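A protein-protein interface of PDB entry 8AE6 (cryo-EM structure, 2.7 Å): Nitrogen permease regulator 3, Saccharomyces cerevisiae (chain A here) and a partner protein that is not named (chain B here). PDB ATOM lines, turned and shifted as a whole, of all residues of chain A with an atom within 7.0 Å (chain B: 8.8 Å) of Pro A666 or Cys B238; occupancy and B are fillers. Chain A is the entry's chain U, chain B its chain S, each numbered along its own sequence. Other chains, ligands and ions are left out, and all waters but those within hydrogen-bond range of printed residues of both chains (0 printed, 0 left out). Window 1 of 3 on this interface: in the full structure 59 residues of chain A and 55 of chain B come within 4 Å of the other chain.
Of the 15 printed residues of chain A, 4 touch a printed residue of chain B. Printed residues of chain A that touch a printed residue of chain B: Lys A663, Leu A664, Pro A666 and Tyr A862. Along chain B the printed residues that touch a printed residue of chain A span positions 236 to 305. Among the printed residues, no Asp or Glu carboxylate lies within 4 Å of a Lys or Arg side-chain nitrogen of the other chain.
O of Lys A663 touches CG2 of Thr B236 (3.2 Å). O of Cys B238 touches CG of Lys A663, 3.3 Å away. Lys A663 touches Asp B243 (CG to OD2, 3.6 Å). Lys A663 touches Leu B305 (O to CD1, 3.4 Å). Leu A664 touches Thr B236. Ile B298 touches Leu A664. Pro A666 touches Thr B236. CG of Pro A666 touches SG of Cys B238, 3.7 Å away. CD1 of Tyr A862 touches SG of Cys B238, at 3.6 Å.
Pro A666 touches just these residues of chain B: Thr B236 and Cys B238. Printed residues of chain A within 4 Å of Cys B238: Lys A663, Pro A666 and Tyr A862. Of the printed residues of chain B, Lys A663 touches Thr B236 (3.2 Å), Cys B238 (3.3 Å), Asp B243 (3.6 Å) and Leu B305 (3.4 Å). Printed residues of chain B within 4 Å of Leu A664: Thr B236 and Ile B298. Ile B291 touches none of the printed residues of chain A. Glu B242 touches none of the printed residues of chain A.
N of Val A667 sits at hydrogen-bond distance from OH of Tyr A862, 3.1 Å away. The side-chain sulfur (SG) of Cys B238 sits at hydrogen-bond distance from the side-chain hydroxyl (OG1) of Thr B236 (2.9 Å). NE of Arg B295 lies within hydrogen-bond range of O of Thr B236 (2.9 Å). The backbone NH (N) of Ser B240 sits at hydrogen-bond distance from the side-chain carboxylate (OD2) of Asp B243 (2.9 Å). The backbone carbonyl oxygen of Asp B243 lies close to the backbone NH of Ile B276, at 3.3 Å.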
ATOM      1  N   GLU A   3      37.288   6.948  -7.138  1.00  0.00           N
ATOM      2  CA  GLU A   3      35.953   6.500  -7.515  1.00  0.00           C
ATOM      3  C   GLU A   3      35.133   6.141  -6.282  1.00  0.00           C
ATOM      4  O   GLU A   3      35.615   5.452  -5.386  1.00  0.00           O
ATOM      5  CB  GLU A   3      36.035   5.303  -8.461  1.00  0.00           C
ATOM      6  CG  GLU A   3      34.707   4.908  -9.082  1.00  0.00           C
ATOM      7  CD  GLU A   3      34.436   5.623 -10.390  1.00  0.00           C
ATOM      8  OE1 GLU A   3      35.341   6.337 -10.875  1.00  0.00           O
ATOM      9  OE2 GLU A   3      33.323   5.473 -10.932  1.00  0.00           O
ATOM     10  N   CYS A   4      33.889   6.615  -6.244  1.00  0.00           N
ATOM     11  CA  CYS A   4      32.993   6.344  -5.130  1.00  0.00           C
ATOM     12  C   CYS A   4      32.203   5.053  -5.298  1.00  0.00           C
ATOM     13  O   CYS A   4      31.603   4.583  -4.327  1.00  0.00           O
ATOM     14  CB  CYS A   4      32.025   7.514  -4.940  1.00  0.00           C
ATOM     15  SG  CYS A   4      32.808   9.028  -4.345  1.00  0.00           S
ATOM     16  N   LEU A   5      32.184   4.477  -6.493  1.00  0.00           N
ATOM     17  CA  LEU A   5      31.523   3.195  -6.691  1.00  0.00           C
ATOM     18  C   LEU A   5      32.360   2.086  -6.062  1.00  0.00           C
ATOM     19  O   LEU A   5      33.584   2.071  -6.234  1.00  0.00           O
ATOM     20  CB  LEU A   5      31.312   2.921  -8.175  1.00  0.00           C
ATOM     21  CG  LEU A   5      30.071   3.539  -8.816  1.00  0.00           C
ATOM     22  CD1 LEU A   5      30.156   3.455 -10.328  1.00  0.00           C
ATOM     23  CD2 LEU A   5      28.815   2.862  -8.310  1.00  0.00           C
ATOM     24  N   PHE A 656      26.612  11.344   1.244  1.00  0.00           N
ATOM     25  CA  PHE A 656      27.163  12.539   0.624  1.00  0.00           C
ATOM     26  C   PHE A 656      26.494  13.773   1.204  1.00  0.00           C
ATOM     27  O   PHE A 656      25.263  13.865   1.221  1.00  0.00           O
ATOM     28  CB  PHE A 656      26.976  12.500  -0.896  1.00  0.00           C
ATOM     29  CG  PHE A 656      27.911  11.563  -1.592  1.00  0.00           C
ATOM     30  CD1 PHE A 656      29.203  11.955  -1.898  1.00  0.00           C
ATOM     31  CD2 PHE A 656      27.502  10.289  -1.939  1.00  0.00           C
ATOM     32  CE1 PHE A 656      30.067  11.092  -2.538  1.00  0.00           C
ATOM     33  CE2 PHE A 656      28.362   9.425  -2.574  1.00  0.00           C
ATOM     34  CZ  PHE A 656      29.644   9.825  -2.875  1.00  0.00           C
ATOM     35  N   PRO A 660      27.160  15.146  -5.392  1.00  0.00           N
ATOM     36  CA  PRO A 660      28.160  14.757  -6.389  1.00  0.00           C
ATOM     37  C   PRO A 660      27.664  15.011  -7.801  1.00  0.00           C
ATOM     38  O   PRO A 660      26.461  15.052  -8.074  1.00  0.00           O
ATOM     39  CB  PRO A 660      28.358  13.262  -6.130  1.00  0.00           C
ATOM     40  CG  PRO A 660      27.077  12.823  -5.528  1.00  0.00           C
ATOM     41  CD  PRO A 660      26.570  13.976  -4.719  1.00  0.00           C
ATOM     42  N   ASN A 661      28.619  15.196  -8.707  1.00  0.00           N
ATOM     43  CA  ASN A 661      28.293  15.391 -10.112  1.00  0.00           C
ATOM     44  C   ASN A 661      27.792  14.079 -10.698  1.00  0.00           C
ATOM     45  O   ASN A 661      28.516  13.080 -10.703  1.00  0.00           O
ATOM     46  CB  ASN A 661      29.513  15.895 -10.874  1.00  0.00           C
ATOM     47  CG  ASN A 661      29.139  16.707 -12.094  1.00  0.00           C
ATOM     48  OD1 ASN A 661      28.057  16.542 -12.656  1.00  0.00           O
ATOM     49  ND2 ASN A 661      30.031  17.597 -12.504  1.00  0.00           N
ATOM     50  N   PHE A 662      26.546  14.082 -11.175  1.00  0.00           N
ATOM     51  CA  PHE A 662      25.918  12.858 -11.664  1.00  0.00           C
ATOM     52  C   PHE A 662      26.601  12.348 -12.924  1.00  0.00           C
ATOM     53  O   PHE A 662      26.956  11.169 -13.022  1.00  0.00           O
ATOM     54  CB  PHE A 662      24.435  13.108 -11.942  1.00  0.00           C
ATOM     55  CG  PHE A 662      23.540  12.853 -10.771  1.00  0.00           C
ATOM     56  CD1 PHE A 662      23.897  13.271  -9.500  1.00  0.00           C
ATOM     57  CD2 PHE A 662      22.332  12.200 -10.943  1.00  0.00           C
ATOM     58  CE1 PHE A 662      23.069  13.037  -8.423  1.00  0.00           C
ATOM     59  CE2 PHE A 662      21.497  11.966  -9.872  1.00  0.00           C
ATOM     60  CZ  PHE A 662      21.869  12.385  -8.611  1.00  0.00           C
ATOM     61  N   LYS A 663      26.797  13.232 -13.900  1.00  0.00           N
ATOM     62  CA  LYS A 663      27.249  12.853 -15.226  1.00  0.00           C
ATOM     63  C   LYS A 663      28.750  13.020 -15.405  1.00  0.00           C
ATOM     64  O   LYS A 663      29.223  13.111 -16.541  1.00  0.00           O
ATOM     65  CB  LYS A 663      26.498  13.662 -16.285  1.00  0.00           C
ATOM     66  CG  LYS A 663      25.230  12.999 -16.797  1.00  0.00           C
ATOM     67  CD  LYS A 663      24.057  13.235 -15.858  1.00  0.00           C
ATOM     68  CE  LYS A 663      23.669  14.702 -15.816  1.00  0.00           C
ATOM     69  NZ  LYS A 663      22.500  14.941 -14.927  1.00  0.00           N
ATOM     70  N   LEU A 664      29.501  13.112 -14.315  1.00  0.00           N
ATOM     71  CA  LEU A 664      30.958  13.115 -14.406  1.00  0.00           C
ATOM     72  C   LEU A 664      31.612  12.113 -13.468  1.00  0.00           C
ATOM     73  O   LEU A 664      32.608  11.492 -13.844  1.00  0.00           O
ATOM     74  CB  LEU A 664      31.507  14.524 -14.135  1.00  0.00           C
ATOM     75  CG  LEU A 664      31.476  15.483 -15.330  1.00  0.00           C
ATOM     76  CD1 LEU A 664      32.191  16.781 -14.999  1.00  0.00           C
ATOM     77  CD2 LEU A 664      32.086  14.839 -16.563  1.00  0.00           C
ATOM     78  N   GLN A 665      31.082  11.938 -12.259  1.00  0.00           N
ATOM     79  CA  GLN A 665      31.557  10.919 -11.325  1.00  0.00           C
ATOM     80  C   GLN A 665      30.380  10.059 -10.868  1.00  0.00           C
ATOM     81  O   GLN A 665      29.530  10.520 -10.088  1.00  0.00           O
ATOM     82  CB  GLN A 665      32.308  11.548 -10.152  1.00  0.00           C
ATOM     83  CG  GLN A 665      31.646  12.752  -9.482  1.00  0.00           C
ATOM     84  CD  GLN A 665      32.470  13.310  -8.339  1.00  0.00           C
ATOM     85  OE1 GLN A 665      33.513  12.760  -7.983  1.00  0.00           O
ATOM     86  NE2 GLN A 665      32.007  14.409  -7.756  1.00  0.00           N
ATOM     87  N   PRO A 666      30.273   8.824 -11.362  1.00  0.00           N
ATOM     88  CA  PRO A 666      29.117   7.990 -11.019  1.00  0.00           C
ATOM     89  C   PRO A 666      29.085   7.614  -9.545  1.00  0.00           C
ATOM     90  O   PRO A 666      30.116   7.342  -8.924  1.00  0.00           O
ATOM     91  CB  PRO A 666      29.294   6.756 -11.909  1.00  0.00           C
ATOM     92  CG  PRO A 666      30.191   7.206 -13.013  1.00  0.00           C
ATOM     93  CD  PRO A 666      31.117   8.200 -12.392  1.00  0.00           C
ATOM     94  N   VAL A 667      27.876   7.604  -8.994  1.00  0.00           N
ATOM     95  CA  VAL A 667      27.603   7.351  -7.585  1.00  0.00           C
ATOM     96  C   VAL A 667      26.452   6.353  -7.532  1.00  0.00           C
ATOM     97  O   VAL A 667      25.567   6.376  -8.391  1.00  0.00           O
ATOM     98  CB  VAL A 667      27.275   8.680  -6.846  1.00  0.00           C
ATOM     99  CG1 VAL A 667      26.614   8.460  -5.502  1.00  0.00           C
ATOM    100  CG2 VAL A 667      28.537   9.511  -6.664  1.00  0.00           C
ATOM    101  N   LEU A 668      26.505   5.438  -6.554  1.00  0.00           N
ATOM    102  CA  LEU A 668      25.464   4.429  -6.355  1.00  0.00           C
ATOM    103  C   LEU A 668      24.078   5.056  -6.267  1.00  0.00           C
ATOM    104  O   LEU A 668      23.856   5.997  -5.503  1.00  0.00           O
ATOM    105  CB  LEU A 668      25.736   3.640  -5.074  1.00  0.00           C
ATOM    106  CG  LEU A 668      26.952   2.729  -4.956  1.00  0.00           C
ATOM    107  CD1 LEU A 668      27.303   2.566  -3.498  1.00  0.00           C
ATOM    108  CD2 LEU A 668      26.669   1.385  -5.580  1.00  0.00           C
ATOM    109  N   ARG A 669      23.156   4.531  -7.067  1.00  0.00           N
ATOM    110  CA  ARG A 669      21.795   5.045  -7.094  1.00  0.00           C
ATOM    111  C   ARG A 669      21.087   4.666  -5.805  1.00  0.00           C
ATOM    112  O   ARG A 669      21.060   3.491  -5.422  1.00  0.00           O
ATOM    113  CB  ARG A 669      21.052   4.492  -8.305  1.00  0.00           C
ATOM    114  CG  ARG A 669      21.782   4.712  -9.614  1.00  0.00           C
ATOM    115  CD  ARG A 669      21.109   3.976 -10.753  1.00  0.00           C
ATOM    116  NE  ARG A 669      21.949   3.926 -11.941  1.00  0.00           N
ATOM    117  CZ  ARG A 669      21.846   4.761 -12.965  1.00  0.00           C
ATOM    118  NH1 ARG A 669      20.949   5.733 -12.975  1.00  0.00           N
ATOM    119  NH2 ARG A 669      22.662   4.618 -14.005  1.00  0.00           N
ATOM    120  N   TYR A 862      24.678   1.796 -14.397  1.00  0.00           N
ATOM    121  CA  TYR A 862      25.314   2.800 -15.262  1.00  0.00           C
ATOM    122  C   TYR A 862      25.663   2.313 -16.673  1.00  0.00           C
ATOM    123  O   TYR A 862      24.926   1.531 -17.270  1.00  0.00           O
ATOM    124  CB  TYR A 862      26.567   3.352 -14.580  1.00  0.00           C
ATOM    125  CG  TYR A 862      26.239   4.357 -13.504  1.00  0.00           C
ATOM    126  CD1 TYR A 862      25.874   5.656 -13.832  1.00  0.00           C
ATOM    127  CD2 TYR A 862      26.271   4.003 -12.163  1.00  0.00           C
ATOM    128  CE1 TYR A 862      25.564   6.576 -12.856  1.00  0.00           C
ATOM    129  CE2 TYR A 862      25.962   4.916 -11.181  1.00  0.00           C
ATOM    130  CZ  TYR A 862      25.609   6.201 -11.532  1.00  0.00           C
ATOM    131  OH  TYR A 862      25.300   7.120 -10.557  1.00  0.00           O
ATOM    132  N   PRO B 234      39.923   8.491 -16.472  1.00  0.00           N
ATOM    133  CA  PRO B 234      39.170   8.298 -17.705  1.00  0.00           C
ATOM    134  C   PRO B 234      37.822   9.000 -17.637  1.00  0.00           C
ATOM    135  O   PRO B 234      37.237   9.140 -16.552  1.00  0.00           O
ATOM    136  CB  PRO B 234      39.000   6.770 -17.784  1.00  0.00           C
ATOM    137  CG  PRO B 234      40.003   6.216 -16.838  1.00  0.00           C
ATOM    138  CD  PRO B 234      40.132   7.226 -15.754  1.00  0.00           C
ATOM    139  N   PRO B 235      37.307   9.470 -18.768  1.00  0.00           N
ATOM    140  CA  PRO B 235      35.978  10.083 -18.773  1.00  0.00           C
ATOM    141  C   PRO B 235      34.880   9.064 -18.532  1.00  0.00           C
ATOM    142  O   PRO B 235      35.013   7.877 -18.840  1.00  0.00           O
ATOM    143  CB  PRO B 235      35.871  10.685 -20.175  1.00  0.00           C
ATOM    144  CG  PRO B 235      36.817   9.897 -20.989  1.00  0.00           C
ATOM    145  CD  PRO B 235      37.956   9.577 -20.080  1.00  0.00           C
ATOM    146  N   THR B 236      33.778   9.554 -17.978  1.00  0.00           N
ATOM    147  CA  THR B 236      32.642   8.721 -17.636  1.00  0.00           C
ATOM    148  C   THR B 236      31.855   8.334 -18.885  1.00  0.00           C
ATOM    149  O   THR B 236      32.021   8.905 -19.966  1.00  0.00           O
ATOM    150  CB  THR B 236      31.732   9.451 -16.662  1.00  0.00           C
ATOM    151  OG1 THR B 236      30.591   8.635 -16.364  1.00  0.00           O
ATOM    152  CG2 THR B 236      31.274  10.739 -17.280  1.00  0.00           C
ATOM    153  N   THR B 237      30.987   7.340 -18.721  1.00  0.00           N
ATOM    154  CA  THR B 237      30.090   6.896 -19.778  1.00  0.00           C
ATOM    155  C   THR B 237      28.671   7.413 -19.583  1.00  0.00           C
ATOM    156  O   THR B 237      27.761   6.988 -20.303  1.00  0.00           O
ATOM    157  CB  THR B 237      30.088   5.371 -19.862  1.00  0.00           C
ATOM    158  OG1 THR B 237      29.751   4.823 -18.581  1.00  0.00           O
ATOM    159  CG2 THR B 237      31.457   4.862 -20.278  1.00  0.00           C
ATOM    160  N   CYS B 238      28.461   8.315 -18.627  1.00  0.00           N
ATOM    161  CA  CYS B 238      27.138   8.828 -18.305  1.00  0.00           C
ATOM    162  C   CYS B 238      26.720   9.996 -19.186  1.00  0.00           C
ATOM    163  O   CYS B 238      25.614  10.516 -19.012  1.00  0.00           O
ATOM    164  CB  CYS B 238      27.082   9.249 -16.835  1.00  0.00           C
ATOM    165  SG  CYS B 238      27.797   8.052 -15.693  1.00  0.00           S
ATOM    166  N   VAL B 239      27.576  10.427 -20.114  1.00  0.00           N
ATOM    167  CA  VAL B 239      27.213  11.504 -21.026  1.00  0.00           C
ATOM    168  C   VAL B 239      26.173  10.993 -22.018  1.00  0.00           C
ATOM    169  O   VAL B 239      26.255   9.860 -22.508  1.00  0.00           O
ATOM    170  CB  VAL B 239      28.473  12.070 -21.707  1.00  0.00           C
ATOM    171  CG1 VAL B 239      29.202  11.018 -22.535  1.00  0.00           C
ATOM    172  CG2 VAL B 239      28.137  13.279 -22.556  1.00  0.00           C
ATOM    173  N   SER B 240      25.145  11.804 -22.261  1.00  0.00           N
ATOM    174  CA  SER B 240      24.012  11.390 -23.075  1.00  0.00           C
ATOM    175  C   SER B 240      23.630  12.539 -24.000  1.00  0.00           C
ATOM    176  O   SER B 240      24.318  13.558 -24.076  1.00  0.00           O
ATOM    177  CB  SER B 240      22.842  10.950 -22.188  1.00  0.00           C
ATOM    178  OG  SER B 240      22.635  11.871 -21.131  1.00  0.00           O
ATOM    179  N   LEU B 241      22.515  12.363 -24.709  1.00  0.00           N
ATOM    180  CA  LEU B 241      22.085  13.335 -25.703  1.00  0.00           C
ATOM    181  C   LEU B 241      21.536  14.608 -25.080  1.00  0.00           C
ATOM    182  O   LEU B 241      21.734  15.696 -25.630  1.00  0.00           O
ATOM    183  CB  LEU B 241      21.028  12.714 -26.614  1.00  0.00           C
ATOM    184  CG  LEU B 241      21.556  11.824 -27.735  1.00  0.00           C
ATOM    185  CD1 LEU B 241      20.428  11.396 -28.656  1.00  0.00           C
ATOM    186  CD2 LEU B 241      22.629  12.555 -28.506  1.00  0.00           C
ATOM    187  N   GLU B 242      20.853  14.504 -23.943  1.00  0.00           N
ATOM    188  CA  GLU B 242      20.203  15.659 -23.344  1.00  0.00           C
ATOM    189  C   GLU B 242      21.166  16.569 -22.599  1.00  0.00           C
ATOM    190  O   GLU B 242      20.769  17.667 -22.199  1.00  0.00           O
ATOM    191  CB  GLU B 242      19.093  15.202 -22.394  1.00  0.00           C
ATOM    192  CG  GLU B 242      19.571  14.829 -21.000  1.00  0.00           C
ATOM    193  CD  GLU B 242      19.825  13.347 -20.843  1.00  0.00           C
ATOM    194  OE1 GLU B 242      19.993  12.656 -21.869  1.00  0.00           O
ATOM    195  OE2 GLU B 242      19.856  12.866 -19.689  1.00  0.00           O
ATOM    196  N   ASP B 243      22.409  16.150 -22.397  1.00  0.00           N
ATOM    197  CA  ASP B 243      23.366  16.972 -21.676  1.00  0.00           C
ATOM    198  C   ASP B 243      23.894  18.075 -22.580  1.00  0.00           C
ATOM    199  O   ASP B 243      24.222  17.840 -23.743  1.00  0.00           O
ATOM    200  CB  ASP B 243      24.523  16.117 -21.162  1.00  0.00           C
ATOM    201  CG  ASP B 243      24.060  15.006 -20.244  1.00  0.00           C
ATOM    202  OD1 ASP B 243      23.090  15.225 -19.484  1.00  0.00           O
ATOM    203  OD2 ASP B 243      24.659  13.912 -20.280  1.00  0.00           O
ATOM    204  N   ILE B 276      23.593  18.061 -26.974  1.00  0.00           N
ATOM    205  CA  ILE B 276      24.456  17.212 -27.787  1.00  0.00           C
ATOM    206  C   ILE B 276      23.718  16.729 -29.032  1.00  0.00           C
ATOM    207  O   ILE B 276      24.316  16.618 -30.109  1.00  0.00           O
ATOM    208  CB  ILE B 276      25.014  16.064 -26.921  1.00  0.00           C
ATOM    209  CG1 ILE B 276      26.169  16.584 -26.070  1.00  0.00           C
ATOM    210  CG2 ILE B 276      25.493  14.879 -27.748  1.00  0.00           C
ATOM    211  CD1 ILE B 276      26.741  15.574 -25.130  1.00  0.00           C
ATOM    212  N   ILE B 291      29.513  12.224 -28.763  1.00  0.00           N
ATOM    213  CA  ILE B 291      29.638  11.730 -27.393  1.00  0.00           C
ATOM    214  C   ILE B 291      31.093  11.406 -27.078  1.00  0.00           C
ATOM    215  O   ILE B 291      31.612  11.779 -26.018  1.00  0.00           O
ATOM    216  CB  ILE B 291      28.717  10.511 -27.186  1.00  0.00           C
ATOM    217  CG1 ILE B 291      27.269  10.955 -26.984  1.00  0.00           C
ATOM    218  CG2 ILE B 291      29.174   9.651 -26.015  1.00  0.00           C
ATOM    219  CD1 ILE B 291      27.063  11.853 -25.801  1.00  0.00           C
ATOM    220  N   ILE B 294      33.120  14.735 -26.833  1.00  0.00           N
ATOM    221  CA  ILE B 294      32.848  15.372 -25.549  1.00  0.00           C
ATOM    222  C   ILE B 294      33.537  14.604 -24.427  1.00  0.00           C
ATOM    223  O   ILE B 294      34.053  15.199 -23.475  1.00  0.00           O
ATOM    224  CB  ILE B 294      31.326  15.492 -25.331  1.00  0.00           C
ATOM    225  CG1 ILE B 294      30.729  16.516 -26.294  1.00  0.00           C
ATOM    226  CG2 ILE B 294      30.983  15.902 -23.907  1.00  0.00           C
ATOM    227  CD1 ILE B 294      31.291  17.910 -26.131  1.00  0.00           C
ATOM    228  N   ARG B 295      33.600  13.274 -24.546  1.00  0.00           N
ATOM    229  CA  ARG B 295      34.323  12.461 -23.570  1.00  0.00           C
ATOM    230  C   ARG B 295      35.818  12.764 -23.588  1.00  0.00           C
ATOM    231  O   ARG B 295      36.453  12.848 -22.531  1.00  0.00           O
ATOM    232  CB  ARG B 295      34.075  10.982 -23.849  1.00  0.00           C
ATOM    233  CG  ARG B 295      32.845  10.421 -23.173  1.00  0.00           C
ATOM    234  CD  ARG B 295      32.684   8.950 -23.481  1.00  0.00           C
ATOM    235  NE  ARG B 295      33.302   8.120 -22.459  1.00  0.00           N
ATOM    236  CZ  ARG B 295      33.925   6.977 -22.703  1.00  0.00           C
ATOM    237  NH1 ARG B 295      34.030   6.496 -23.931  1.00  0.00           N
ATOM    238  NH2 ARG B 295      34.458   6.298 -21.692  1.00  0.00           N
ATOM    239  N   ILE B 298      36.301  15.998 -21.922  1.00  0.00           N
ATOM    240  CA  ILE B 298      36.170  15.787 -20.483  1.00  0.00           C
ATOM    241  C   ILE B 298      37.469  15.235 -19.913  1.00  0.00           C
ATOM    242  O   ILE B 298      37.908  15.628 -18.824  1.00  0.00           O
ATOM    243  CB  ILE B 298      34.969  14.859 -20.201  1.00  0.00           C
ATOM    244  CG1 ILE B 298      33.658  15.639 -20.269  1.00  0.00           C
ATOM    245  CG2 ILE B 298      35.078  14.165 -18.849  1.00  0.00           C
ATOM    246  CD1 ILE B 298      32.458  14.778 -20.564  1.00  0.00           C
ATOM    247  N   LEU B 305      29.450  19.003 -18.248  1.00  0.00           N
ATOM    248  CA  LEU B 305      28.094  18.825 -18.736  1.00  0.00           C
ATOM    249  C   LEU B 305      27.094  19.602 -17.880  1.00  0.00           C
ATOM    250  O   LEU B 305      27.335  19.903 -16.710  1.00  0.00           O
ATOM    251  CB  LEU B 305      27.723  17.346 -18.749  1.00  0.00           C
ATOM    252  CG  LEU B 305      28.618  16.460 -19.608  1.00  0.00           C
ATOM    253  CD1 LEU B 305      28.404  15.005 -19.250  1.00  0.00           C
ATOM    254  CD2 LEU B 305      28.345  16.703 -21.078  1.00  0.00           C
ATOM    255  N   LYS B 588      15.105  13.653 -21.880  1.00  0.00           N
ATOM    256  CA  LYS B 588      15.576  12.666 -22.845  1.00  0.00           C
ATOM    257  C   LYS B 588      14.493  12.308 -23.855  1.00  0.00           C
ATOM    258  O   LYS B 588      14.781  12.149 -25.045  1.00  0.00           O
ATOM    259  CB  LYS B 588      16.072  11.417 -22.120  1.00  0.00           C
ATOM    260  CG  LYS B 588      16.815  10.433 -23.009  1.00  0.00           C
ATOM    261  CD  LYS B 588      17.865  11.119 -23.866  1.00  0.00           C
ATOM    262  CE  LYS B 588      18.612  10.119 -24.728  1.00  0.00           C
ATOM    263  NZ  LYS B 588      19.353   9.124 -23.904  1.00  0.00           N
